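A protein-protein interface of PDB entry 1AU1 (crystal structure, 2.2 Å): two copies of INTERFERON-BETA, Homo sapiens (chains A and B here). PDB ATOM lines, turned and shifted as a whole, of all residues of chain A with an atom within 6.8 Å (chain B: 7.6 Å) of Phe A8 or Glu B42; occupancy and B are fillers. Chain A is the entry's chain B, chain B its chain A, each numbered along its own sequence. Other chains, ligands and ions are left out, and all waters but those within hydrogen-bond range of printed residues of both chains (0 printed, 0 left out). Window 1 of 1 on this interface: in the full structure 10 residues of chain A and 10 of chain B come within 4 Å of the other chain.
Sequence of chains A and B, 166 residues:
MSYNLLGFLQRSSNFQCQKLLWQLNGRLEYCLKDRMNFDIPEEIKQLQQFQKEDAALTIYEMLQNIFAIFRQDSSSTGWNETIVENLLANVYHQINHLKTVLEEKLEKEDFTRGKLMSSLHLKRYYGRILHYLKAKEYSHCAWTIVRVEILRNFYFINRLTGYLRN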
ATOM      1  N   SER A   2      14.653   9.561  15.281  1.00  0.00           N
ATOM      2  CA  SER A   2      15.144   8.845  14.132  1.00  0.00           C
ATOM      3  C   SER A   2      16.532   9.439  13.938  1.00  0.00           C
ATOM      4  O   SER A   2      17.352   8.876  13.219  1.00  0.00           O
ATOM      5  CB  SER A   2      14.168   8.876  12.857  1.00  0.00           C
ATOM      6  OG  SER A   2      14.316   9.982  12.018  1.00  0.00           O
ATOM      7  N   TYR A   3      16.822  10.477  14.734  1.00  0.00           N
ATOM      8  CA  TYR A   3      18.162  11.092  14.764  1.00  0.00           C
ATOM      9  C   TYR A   3      19.110  10.226  15.546  1.00  0.00           C
ATOM     10  O   TYR A   3      20.296  10.323  15.343  1.00  0.00           O
ATOM     11  CB  TYR A   3      18.161  12.514  15.327  1.00  0.00           C
ATOM     12  CG  TYR A   3      18.062  13.599  14.250  1.00  0.00           C
ATOM     13  CD1 TYR A   3      19.199  14.069  13.582  1.00  0.00           C
ATOM     14  CD2 TYR A   3      16.825  14.091  13.849  1.00  0.00           C
ATOM     15  CE1 TYR A   3      19.097  14.996  12.523  1.00  0.00           C
ATOM     16  CE2 TYR A   3      16.707  15.011  12.804  1.00  0.00           C
ATOM     17  CZ  TYR A   3      17.838  15.464  12.137  1.00  0.00           C
ATOM     18  OH  TYR A   3      17.672  16.385  11.101  1.00  0.00           O
ATOM     19  N   ASN A   4      18.587   9.403  16.451  1.00  0.00           N
ATOM     20  CA  ASN A   4      19.469   8.506  17.176  1.00  0.00           C
ATOM     21  C   ASN A   4      19.834   7.362  16.263  1.00  0.00           C
ATOM     22  O   ASN A   4      21.014   6.972  16.198  1.00  0.00           O
ATOM     23  CB  ASN A   4      18.869   8.023  18.497  1.00  0.00           C
ATOM     24  CG  ASN A   4      19.219   8.955  19.655  1.00  0.00           C
ATOM     25  OD1 ASN A   4      20.388   9.165  19.970  1.00  0.00           O
ATOM     26  ND2 ASN A   4      18.212   9.560  20.253  1.00  0.00           N
ATOM     27  N   LEU A   5      18.859   6.837  15.520  1.00  0.00           N
ATOM     28  CA  LEU A   5      19.218   5.758  14.609  1.00  0.00           C
ATOM     29  C   LEU A   5      20.068   6.319  13.472  1.00  0.00           C
ATOM     30  O   LEU A   5      21.022   5.693  13.048  1.00  0.00           O
ATOM     31  CB  LEU A   5      18.001   5.018  14.077  1.00  0.00           C
ATOM     32  CG  LEU A   5      18.361   3.964  13.013  1.00  0.00           C
ATOM     33  CD1 LEU A   5      19.342   2.959  13.512  1.00  0.00           C
ATOM     34  CD2 LEU A   5      17.161   3.257  12.555  1.00  0.00           C
ATOM     35  N   LEU A   6      19.752   7.525  13.023  1.00  0.00           N
ATOM     36  CA  LEU A   6      20.514   8.149  11.963  1.00  0.00           C
ATOM     37  C   LEU A   6      21.959   8.317  12.353  1.00  0.00           C
ATOM     38  O   LEU A   6      22.844   7.972  11.592  1.00  0.00           O
ATOM     39  CB  LEU A   6      19.941   9.508  11.589  1.00  0.00           C
ATOM     40  CG  LEU A   6      20.754  10.263  10.506  1.00  0.00           C
ATOM     41  CD1 LEU A   6      20.730   9.555   9.165  1.00  0.00           C
ATOM     42  CD2 LEU A   6      20.175  11.659  10.365  1.00  0.00           C
ATOM     43  N   GLY A   7      22.199   8.913  13.508  1.00  0.00           N
ATOM     44  CA  GLY A   7      23.556   9.118  13.984  1.00  0.00           C
ATOM     45  C   GLY A   7      24.277   7.796  14.161  1.00  0.00           C
ATOM     46  O   GLY A   7      25.498   7.708  13.959  1.00  0.00           O
ATOM     47  N   PHE A   8      23.540   6.749  14.532  1.00  0.00           N
ATOM     48  CA  PHE A   8      24.141   5.436  14.708  1.00  0.00           C
ATOM     49  C   PHE A   8      24.596   5.018  13.331  1.00  0.00           C
ATOM     50  O   PHE A   8      25.776   4.740  13.126  1.00  0.00           O
ATOM     51  CB  PHE A   8      23.153   4.410  15.279  1.00  0.00           C
ATOM     52  CG  PHE A   8      23.705   3.007  15.315  1.00  0.00           C
ATOM     53  CD1 PHE A   8      23.615   2.175  14.190  1.00  0.00           C
ATOM     54  CD2 PHE A   8      24.372   2.525  16.440  1.00  0.00           C
ATOM     55  CE1 PHE A   8      24.174   0.876  14.181  1.00  0.00           C
ATOM     56  CE2 PHE A   8      24.930   1.229  16.440  1.00  0.00           C
ATOM     57  CZ  PHE A   8      24.833   0.409  15.304  1.00  0.00           C
ATOM     58  N   LEU A   9      23.675   5.044  12.370  1.00  0.00           N
ATOM     59  CA  LEU A   9      23.984   4.663  10.993  1.00  0.00           C
ATOM     60  C   LEU A   9      25.085   5.546  10.440  1.00  0.00           C
ATOM     61  O   LEU A   9      25.955   5.059   9.729  1.00  0.00           O
ATOM     62  CB  LEU A   9      22.734   4.709  10.106  1.00  0.00           C
ATOM     63  CG  LEU A   9      21.590   3.768  10.501  1.00  0.00           C
ATOM     64  CD1 LEU A   9      20.309   3.960   9.694  1.00  0.00           C
ATOM     65  CD2 LEU A   9      22.087   2.370  10.411  1.00  0.00           C
ATOM     66  N   GLN A  10      25.136   6.801  10.870  1.00  0.00           N
ATOM     67  CA  GLN A  10      26.181   7.675  10.390  1.00  0.00           C
ATOM     68  C   GLN A  10      27.553   7.337  10.929  1.00  0.00           C
ATOM     69  O   GLN A  10      28.535   7.463  10.205  1.00  0.00           O
ATOM     70  CB  GLN A  10      25.890   9.113  10.683  1.00  0.00           C
ATOM     71  CG  GLN A  10      26.891  10.013  10.022  1.00  0.00           C
ATOM     72  CD  GLN A  10      26.700  10.107   8.509  1.00  0.00           C
ATOM     73  OE1 GLN A  10      25.570  10.174   8.029  1.00  0.00           O
ATOM     74  NE2 GLN A  10      27.794  10.109   7.758  1.00  0.00           N
ATOM     75  N   ARG A  11      27.657   6.958  12.198  1.00  0.00           N
ATOM     76  CA  ARG A  11      28.966   6.590  12.749  1.00  0.00           C
ATOM     77  C   ARG A  11      29.508   5.338  12.036  1.00  0.00           C
ATOM     78  O   ARG A  11      30.698   5.207  11.742  1.00  0.00           O
ATOM     79  CB  ARG A  11      28.862   6.316  14.241  1.00  0.00           C
ATOM     80  CG  ARG A  11      28.503   7.505  15.092  1.00  0.00           C
ATOM     81  CD  ARG A  11      28.606   7.148  16.552  1.00  0.00           C
ATOM     82  NE  ARG A  11      27.389   6.532  17.050  1.00  0.00           N
ATOM     83  CZ  ARG A  11      26.282   7.214  17.302  1.00  0.00           C
ATOM     84  NH1 ARG A  11      26.234   8.524  17.090  1.00  0.00           N
ATOM     85  NH2 ARG A  11      25.237   6.596  17.822  1.00  0.00           N
ATOM     86  N   SER A  12      28.589   4.429  11.742  1.00  0.00           N
ATOM     87  CA  SER A  12      28.847   3.168  11.056  1.00  0.00           C
ATOM     88  C   SER A  12      29.432   3.413   9.663  1.00  0.00           C
ATOM     89  O   SER A  12      30.370   2.741   9.245  1.00  0.00           O
ATOM     90  CB  SER A  12      27.513   2.432  10.941  1.00  0.00           C
ATOM     91  OG  SER A  12      27.643   1.056  11.223  1.00  0.00           O
ATOM     92  N   SER A  13      28.821   4.350   8.943  1.00  0.00           N
ATOM     93  CA  SER A  13      29.243   4.769   7.607  1.00  0.00           C
ATOM     94  C   SER A  13      30.596   5.520   7.665  1.00  0.00           C
ATOM     95  O   SER A  13      31.497   5.284   6.855  1.00  0.00           O
ATOM     96  CB  SER A  13      28.155   5.663   6.976  1.00  0.00           C
ATOM     97  OG  SER A  13      28.484   6.085   5.651  1.00  0.00           O
ATOM     98  N   GLN A  16      33.375   2.783   8.163  1.00  0.00           N
ATOM     99  CA  GLN A  16      33.654   1.996   6.975  1.00  0.00           C
ATOM    100  C   GLN A  16      34.350   2.822   5.899  1.00  0.00           C
ATOM    101  O   GLN A  16      35.381   2.432   5.400  1.00  0.00           O
ATOM    102  CB  GLN A  16      32.359   1.401   6.408  1.00  0.00           C
ATOM    103  CG  GLN A  16      31.609   0.499   7.376  1.00  0.00           C
ATOM    104  CD  GLN A  16      32.361  -0.795   7.718  1.00  0.00           C
ATOM    105  OE1 GLN A  16      33.522  -0.969   7.344  1.00  0.00           O
ATOM    106  NE2 GLN A  16      31.672  -1.735   8.368  1.00  0.00           N
ATOM    107  N   GLN A  94      24.095   5.747   2.586  1.00  0.00           N
ATOM    108  CA  GLN A  94      23.976   6.733   3.660  1.00  0.00           C
ATOM    109  C   GLN A  94      23.378   8.056   3.184  1.00  0.00           C
ATOM    110  O   GLN A  94      22.594   8.683   3.901  1.00  0.00           O
ATOM    111  CB  GLN A  94      25.317   6.932   4.376  1.00  0.00           C
ATOM    112  CG  GLN A  94      25.290   7.809   5.651  1.00  0.00           C
ATOM    113  CD  GLN A  94      24.432   7.258   6.787  1.00  0.00           C
ATOM    114  OE1 GLN A  94      24.080   6.078   6.825  1.00  0.00           O
ATOM    115  NE2 GLN A  94      24.066   8.130   7.702  1.00  0.00           N
ATOM    116  N   THR A 161      28.853  14.703  12.820  1.00  0.00           N
ATOM    117  CA  THR A 161      28.061  13.510  13.160  1.00  0.00           C
ATOM    118  C   THR A 161      27.761  13.460  14.650  1.00  0.00           C
ATOM    119  O   THR A 161      26.876  12.718  15.099  1.00  0.00           O
ATOM    120  CB  THR A 161      28.787  12.223  12.768  1.00  0.00           C
ATOM    121  OG1 THR A 161      28.895  12.208  11.347  1.00  0.00           O
ATOM    122  CG2 THR A 161      28.067  10.981  13.249  1.00  0.00           C
ATOM    123  N   LEU A 164      24.263  14.681  15.536  1.00  0.00           N
ATOM    124  CA  LEU A 164      23.182  13.835  15.055  1.00  0.00           C
ATOM    125  C   LEU A 164      22.570  13.027  16.182  1.00  0.00           C
ATOM    126  O   LEU A 164      22.681  11.798  16.214  1.00  0.00           O
ATOM    127  CB  LEU A 164      23.696  12.907  13.947  1.00  0.00           C
ATOM    128  CG  LEU A 164      24.115  13.661  12.685  1.00  0.00           C
ATOM    129  CD1 LEU A 164      24.371  12.654  11.613  1.00  0.00           C
ATOM    130  CD2 LEU A 164      23.035  14.664  12.262  1.00  0.00           C
ATOM    131  N   ASP B  39      24.326 -11.865   8.267  1.00  0.00           N
ATOM    132  CA  ASP B  39      24.484 -10.503   8.768  1.00  0.00           C
ATOM    133  C   ASP B  39      23.238  -9.797   9.242  1.00  0.00           C
ATOM    134  O   ASP B  39      22.687  -8.962   8.543  1.00  0.00           O
ATOM    135  CB  ASP B  39      25.184  -9.616   7.752  1.00  0.00           C
ATOM    136  CG  ASP B  39      26.461 -10.234   7.203  1.00  0.00           C
ATOM    137  OD1 ASP B  39      27.204 -10.920   7.945  1.00  0.00           O
ATOM    138  OD2 ASP B  39      26.712 -10.033   5.998  1.00  0.00           O
ATOM    139  N   ILE B  40      22.828 -10.088  10.462  1.00  0.00           N
ATOM    140  CA  ILE B  40      21.654  -9.454  11.013  1.00  0.00           C
ATOM    141  C   ILE B  40      22.034  -7.973  11.064  1.00  0.00           C
ATOM    142  O   ILE B  40      23.194  -7.631  11.300  1.00  0.00           O
ATOM    143  CB  ILE B  40      21.276 -10.108  12.400  1.00  0.00           C
ATOM    144  CG1 ILE B  40      19.909  -9.599  12.898  1.00  0.00           C
ATOM    145  CG2 ILE B  40      22.365  -9.911  13.388  1.00  0.00           C
ATOM    146  CD1 ILE B  40      19.280 -10.453  14.024  1.00  0.00           C
ATOM    147  N   PRO B  41      21.078  -7.072  10.728  1.00  0.00           N
ATOM    148  CA  PRO B  41      21.449  -5.650  10.760  1.00  0.00           C
ATOM    149  C   PRO B  41      22.103  -5.258  12.055  1.00  0.00           C
ATOM    150  O   PRO B  41      21.656  -5.575  13.140  1.00  0.00           O
ATOM    151  CB  PRO B  41      20.117  -4.937  10.574  1.00  0.00           C
ATOM    152  CG  PRO B  41      19.307  -5.907   9.825  1.00  0.00           C
ATOM    153  CD  PRO B  41      19.664  -7.243  10.411  1.00  0.00           C
ATOM    154  N   GLU B  42      23.197  -4.551  11.897  1.00  0.00           N
ATOM    155  CA  GLU B  42      24.017  -4.050  12.978  1.00  0.00           C
ATOM    156  C   GLU B  42      23.237  -3.292  14.096  1.00  0.00           C
ATOM    157  O   GLU B  42      23.607  -3.323  15.266  1.00  0.00           O
ATOM    158  CB  GLU B  42      25.080  -3.157  12.312  1.00  0.00           C
ATOM    159  CG  GLU B  42      26.269  -2.762  13.145  1.00  0.00           C
ATOM    160  CD  GLU B  42      27.055  -1.644  12.493  1.00  0.00           C
ATOM    161  OE1 GLU B  42      26.854  -1.410  11.276  1.00  0.00           O
ATOM    162  OE2 GLU B  42      27.864  -0.994  13.196  1.00  0.00           O
ATOM    163  N   GLU B  43      22.164  -2.601  13.749  1.00  0.00           N
ATOM    164  CA  GLU B  43      21.421  -1.858  14.758  1.00  0.00           C
ATOM    165  C   GLU B  43      20.630  -2.773  15.685  1.00  0.00           C
ATOM    166  O   GLU B  43      20.406  -2.464  16.847  1.00  0.00           O
ATOM    167  CB  GLU B  43      20.496  -0.807  14.120  1.00  0.00           C
ATOM    168  CG  GLU B  43      19.379  -1.345  13.211  1.00  0.00           C
ATOM    169  CD  GLU B  43      19.786  -1.464  11.751  1.00  0.00           C
ATOM    170  OE1 GLU B  43      20.968  -1.533  11.431  1.00  0.00           O
ATOM    171  OE2 GLU B  43      18.913  -1.499  10.885  1.00  0.00           O
ATOM    172  N   ILE B  44      20.250  -3.933  15.184  1.00  0.00           N
ATOM    173  CA  ILE B  44      19.476  -4.865  15.977  1.00  0.00           C
ATOM    174  C   ILE B  44      20.315  -5.380  17.125  1.00  0.00           C
ATOM    175  O   ILE B  44      19.798  -5.768  18.171  1.00  0.00           O
ATOM    176  CB  ILE B  44      18.987  -6.048  15.113  1.00  0.00           C
ATOM    177  CG1 ILE B  44      18.006  -5.553  14.030  1.00  0.00           C
ATOM    178  CG2 ILE B  44      18.404  -7.162  15.996  1.00  0.00           C
ATOM    179  CD1 ILE B  44      16.741  -4.910  14.538  1.00  0.00           C
ATOM    180  N   LYS B  45      21.623  -5.376  16.922  1.00  0.00           N
ATOM    181  CA  LYS B  45      22.534  -5.840  17.939  1.00  0.00           C
ATOM    182  C   LYS B  45      23.180  -4.720  18.753  1.00  0.00           C
ATOM    183  O   LYS B  45      23.388  -4.851  19.967  1.00  0.00           O
ATOM    184  CB  LYS B  45      23.634  -6.654  17.289  1.00  0.00           C
ATOM    185  CG  LYS B  45      23.139  -7.693  16.355  1.00  0.00           C
ATOM    186  CD  LYS B  45      24.289  -8.481  15.814  1.00  0.00           C
ATOM    187  CE  LYS B  45      25.255  -7.582  15.082  1.00  0.00           C
ATOM    188  NZ  LYS B  45      26.404  -8.356  14.547  1.00  0.00           N
ATOM    189  N   GLN B  46      23.513  -3.623  18.093  1.00  0.00           N
ATOM    190  CA  GLN B  46      24.193  -2.568  18.795  1.00  0.00           C
ATOM    191  C   GLN B  46      23.481  -1.287  19.102  1.00  0.00           C
ATOM    192  O   GLN B  46      23.976  -0.524  19.912  1.00  0.00           O
ATOM    193  CB  GLN B  46      25.483  -2.244  18.080  1.00  0.00           C
ATOM    194  CG  GLN B  46      26.517  -3.304  18.197  1.00  0.00           C
ATOM    195  CD  GLN B  46      27.763  -2.956  17.407  1.00  0.00           C
ATOM    196  OE1 GLN B  46      28.013  -1.795  17.060  1.00  0.00           O
ATOM    197  NE2 GLN B  46      28.569  -3.964  17.135  1.00  0.00           N
ATOM    198  N   LEU B  47      22.353  -1.007  18.468  1.00  0.00           N
ATOM    199  CA  LEU B  47      21.695   0.254  18.754  1.00  0.00           C
ATOM    200  C   LEU B  47      21.324   0.334  20.241  1.00  0.00           C
ATOM    201  O   LEU B  47      20.670  -0.569  20.759  1.00  0.00           O
ATOM    202  CB  LEU B  47      20.469   0.464  17.856  1.00  0.00           C
ATOM    203  CG  LEU B  47      19.766   1.829  18.012  1.00  0.00           C
ATOM    204  CD1 LEU B  47      20.711   2.926  17.608  1.00  0.00           C
ATOM    205  CD2 LEU B  47      18.510   1.908  17.193  1.00  0.00           C
ATOM    206  N   GLN B  48      21.738   1.426  20.902  1.00  0.00           N
ATOM    207  CA  GLN B  48      21.505   1.660  22.342  1.00  0.00           C
ATOM    208  C   GLN B  48      20.251   2.439  22.714  1.00  0.00           C
ATOM    209  O   GLN B  48      19.768   2.370  23.830  1.00  0.00           O
ATOM    210  CB  GLN B  48      22.698   2.396  22.967  1.00  0.00           C
ATOM    211  CG  GLN B  48      24.070   1.820  22.711  1.00  0.00           C
ATOM    212  CD  GLN B  48      24.193   0.374  23.153  1.00  0.00           C
ATOM    213  OE1 GLN B  48      25.044  -0.367  22.647  1.00  0.00           O
ATOM    214  NE2 GLN B  48      23.292  -0.066  24.035  1.00  0.00           N
ATOM    215  N   GLN B  49      19.760   3.244  21.790  1.00  0.00           N
ATOM    216  CA  GLN B  49      18.592   4.082  22.058  1.00  0.00           C
ATOM    217  C   GLN B  49      17.375   3.643  21.291  1.00  0.00           C
ATOM    218  O   GLN B  49      17.248   3.982  20.106  1.00  0.00           O
ATOM    219  CB  GLN B  49      18.909   5.540  21.707  1.00  0.00           C
ATOM    220  CG  GLN B  49      20.054   6.142  22.501  1.00  0.00           C
ATOM    221  CD  GLN B  49      19.786   6.116  23.999  1.00  0.00           C
ATOM    222  OE1 GLN B  49      18.826   6.726  24.468  1.00  0.00           O
ATOM    223  NE2 GLN B  49      20.624   5.403  24.753  1.00  0.00           N
ATOM    224  N   MET B 117      14.071   1.698  12.391  1.00  0.00           N
ATOM    225  CA  MET B 117      15.079   0.684  12.722  1.00  0.00           C
ATOM    226  C   MET B 117      14.738  -0.610  11.980  1.00  0.00           C
ATOM    227  O   MET B 117      15.598  -1.251  11.370  1.00  0.00           O
ATOM    228  CB  MET B 117      15.040   0.445  14.214  1.00  0.00           C
ATOM    229  CG  MET B 117      16.037  -0.635  14.653  1.00  0.00           C
ATOM    230  SD  MET B 117      16.018  -0.905  16.431  1.00  0.00           S
ATOM    231  CE  MET B 117      17.273  -2.193  16.498  1.00  0.00           C
ATOM    232  N   HIS B 121      16.356  -2.600   6.764  1.00  0.00           N
ATOM    233  CA  HIS B 121      17.290  -3.698   6.775  1.00  0.00           C
ATOM    234  C   HIS B 121      16.754  -5.059   7.159  1.00  0.00           C
ATOM    235  O   HIS B 121      17.333  -6.069   6.766  1.00  0.00           O
ATOM    236  CB  HIS B 121      18.489  -3.305   7.611  1.00  0.00           C
ATOM    237  CG  HIS B 121      19.071  -1.981   7.212  1.00  0.00           C
ATOM    238  ND1 HIS B 121      19.353  -0.964   8.085  1.00  0.00           N
ATOM    239  CD2 HIS B 121      19.394  -1.503   5.986  1.00  0.00           C
ATOM    240  CE1 HIS B 121      19.829   0.075   7.374  1.00  0.00           C
ATOM    241  NE2 HIS B 121      19.872  -0.206   6.089  1.00  0.00           N
ATOM    242  N   ARG B 159      17.032  -8.945  23.890  1.00  0.00           N
ATOM    243  CA  ARG B 159      17.740  -7.704  24.195  1.00  0.00           C
ATOM    244  C   ARG B 159      16.765  -6.579  23.924  1.00  0.00           C
ATOM    245  O   ARG B 159      16.623  -5.659  24.727  1.00  0.00           O
ATOM    246  CB  ARG B 159      18.963  -7.535  23.285  1.00  0.00           C
ATOM    247  CG  ARG B 159      19.819  -6.313  23.601  1.00  0.00           C
ATOM    248  CD  ARG B 159      20.885  -6.107  22.540  1.00  0.00           C
ATOM    249  NE  ARG B 159      20.442  -5.300  21.391  1.00  0.00           N
ATOM    250  CZ  ARG B 159      20.559  -3.971  21.295  1.00  0.00           C
ATOM    251  NH1 ARG B 159      21.090  -3.262  22.276  1.00  0.00           N
ATOM    252  NH2 ARG B 159      20.222  -3.350  20.180  1.00  0.00           N
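Of the 14 printed residues of chain B, 6 touch a printed residue of chain A.
Hydrophobic or aromatic side chains of chain B that line the printed part of chain A: Leu B47 and Met B117.
Printed residues of chain A that touch a printed residue of chain B: Asn A4, Leu A5, Phe A8 and Ser A12.
Hydrophobic or aromatic side chains of chain A within 4 Å of the printed part of chain B: Leu A5 and Phe A8.
ND1 of His B121 is in hydrogen-bond range of OE2 of Glu B43 (2.9 Å).
The backbone carbonyl oxygen (O) of Glu B43 lies within hydrogen-bond range of the guanidinium group (NH2) of Arg B159 (3.5 Å).
The backbone carbonyl oxygen (O) of Gln B46 lies close to the side-chain amide oxygen (OE1) of Gln B48 (2.9 Å).
The backbone carbonyl oxygen (O) of Leu B47 sits at hydrogen-bond distance from the guanidinium group (NH2) of Arg B159 (2.9 Å).
OD1 of Asn A4 touches CG of Gln B49 (3.96 Å).
Glu B43 touches Leu A5 (CB to CD1, 3.99 Å).
Leu A5 touches Leu B47 (CD1 to CD2, 3.9 Å).
Met B117 touches Leu A5.
Phe A8 touches Glu B42 (CZ to O, 3.9 Å).
Glu B43 touches Phe A8.
Gln B46 touches Phe A8 (CB to CE2, 3.9 Å).
CB of Phe A8 touches CD1 of Leu B47, at 3.7 Å.
No position is printed for both chains.
Of the 9 pairs that touch across the chains among the printed residues, none has its exchanged pair printed and touching as well.
Of the printed residues of chain B, Asn A4 touches Gln B49 (3.96 Å).
No residue of chain B comes within 4 Å of Gly A7.
Leu A9 touches none of the printed residues of chain B.
Gln A94 touches none of the printed residues of chain B.
Of chain A, only Phe A8 (3.9 Å) and Ser A12 (2.6 Å) come within 4 Å of Glu B42.
Of the printed residues of chain A, Gln B49 touches Asn A4.
The side-chain carboxylate (OE1) of Glu B42 lies within hydrogen-bond range of the side-chain hydroxyl (OG) of Ser A12.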
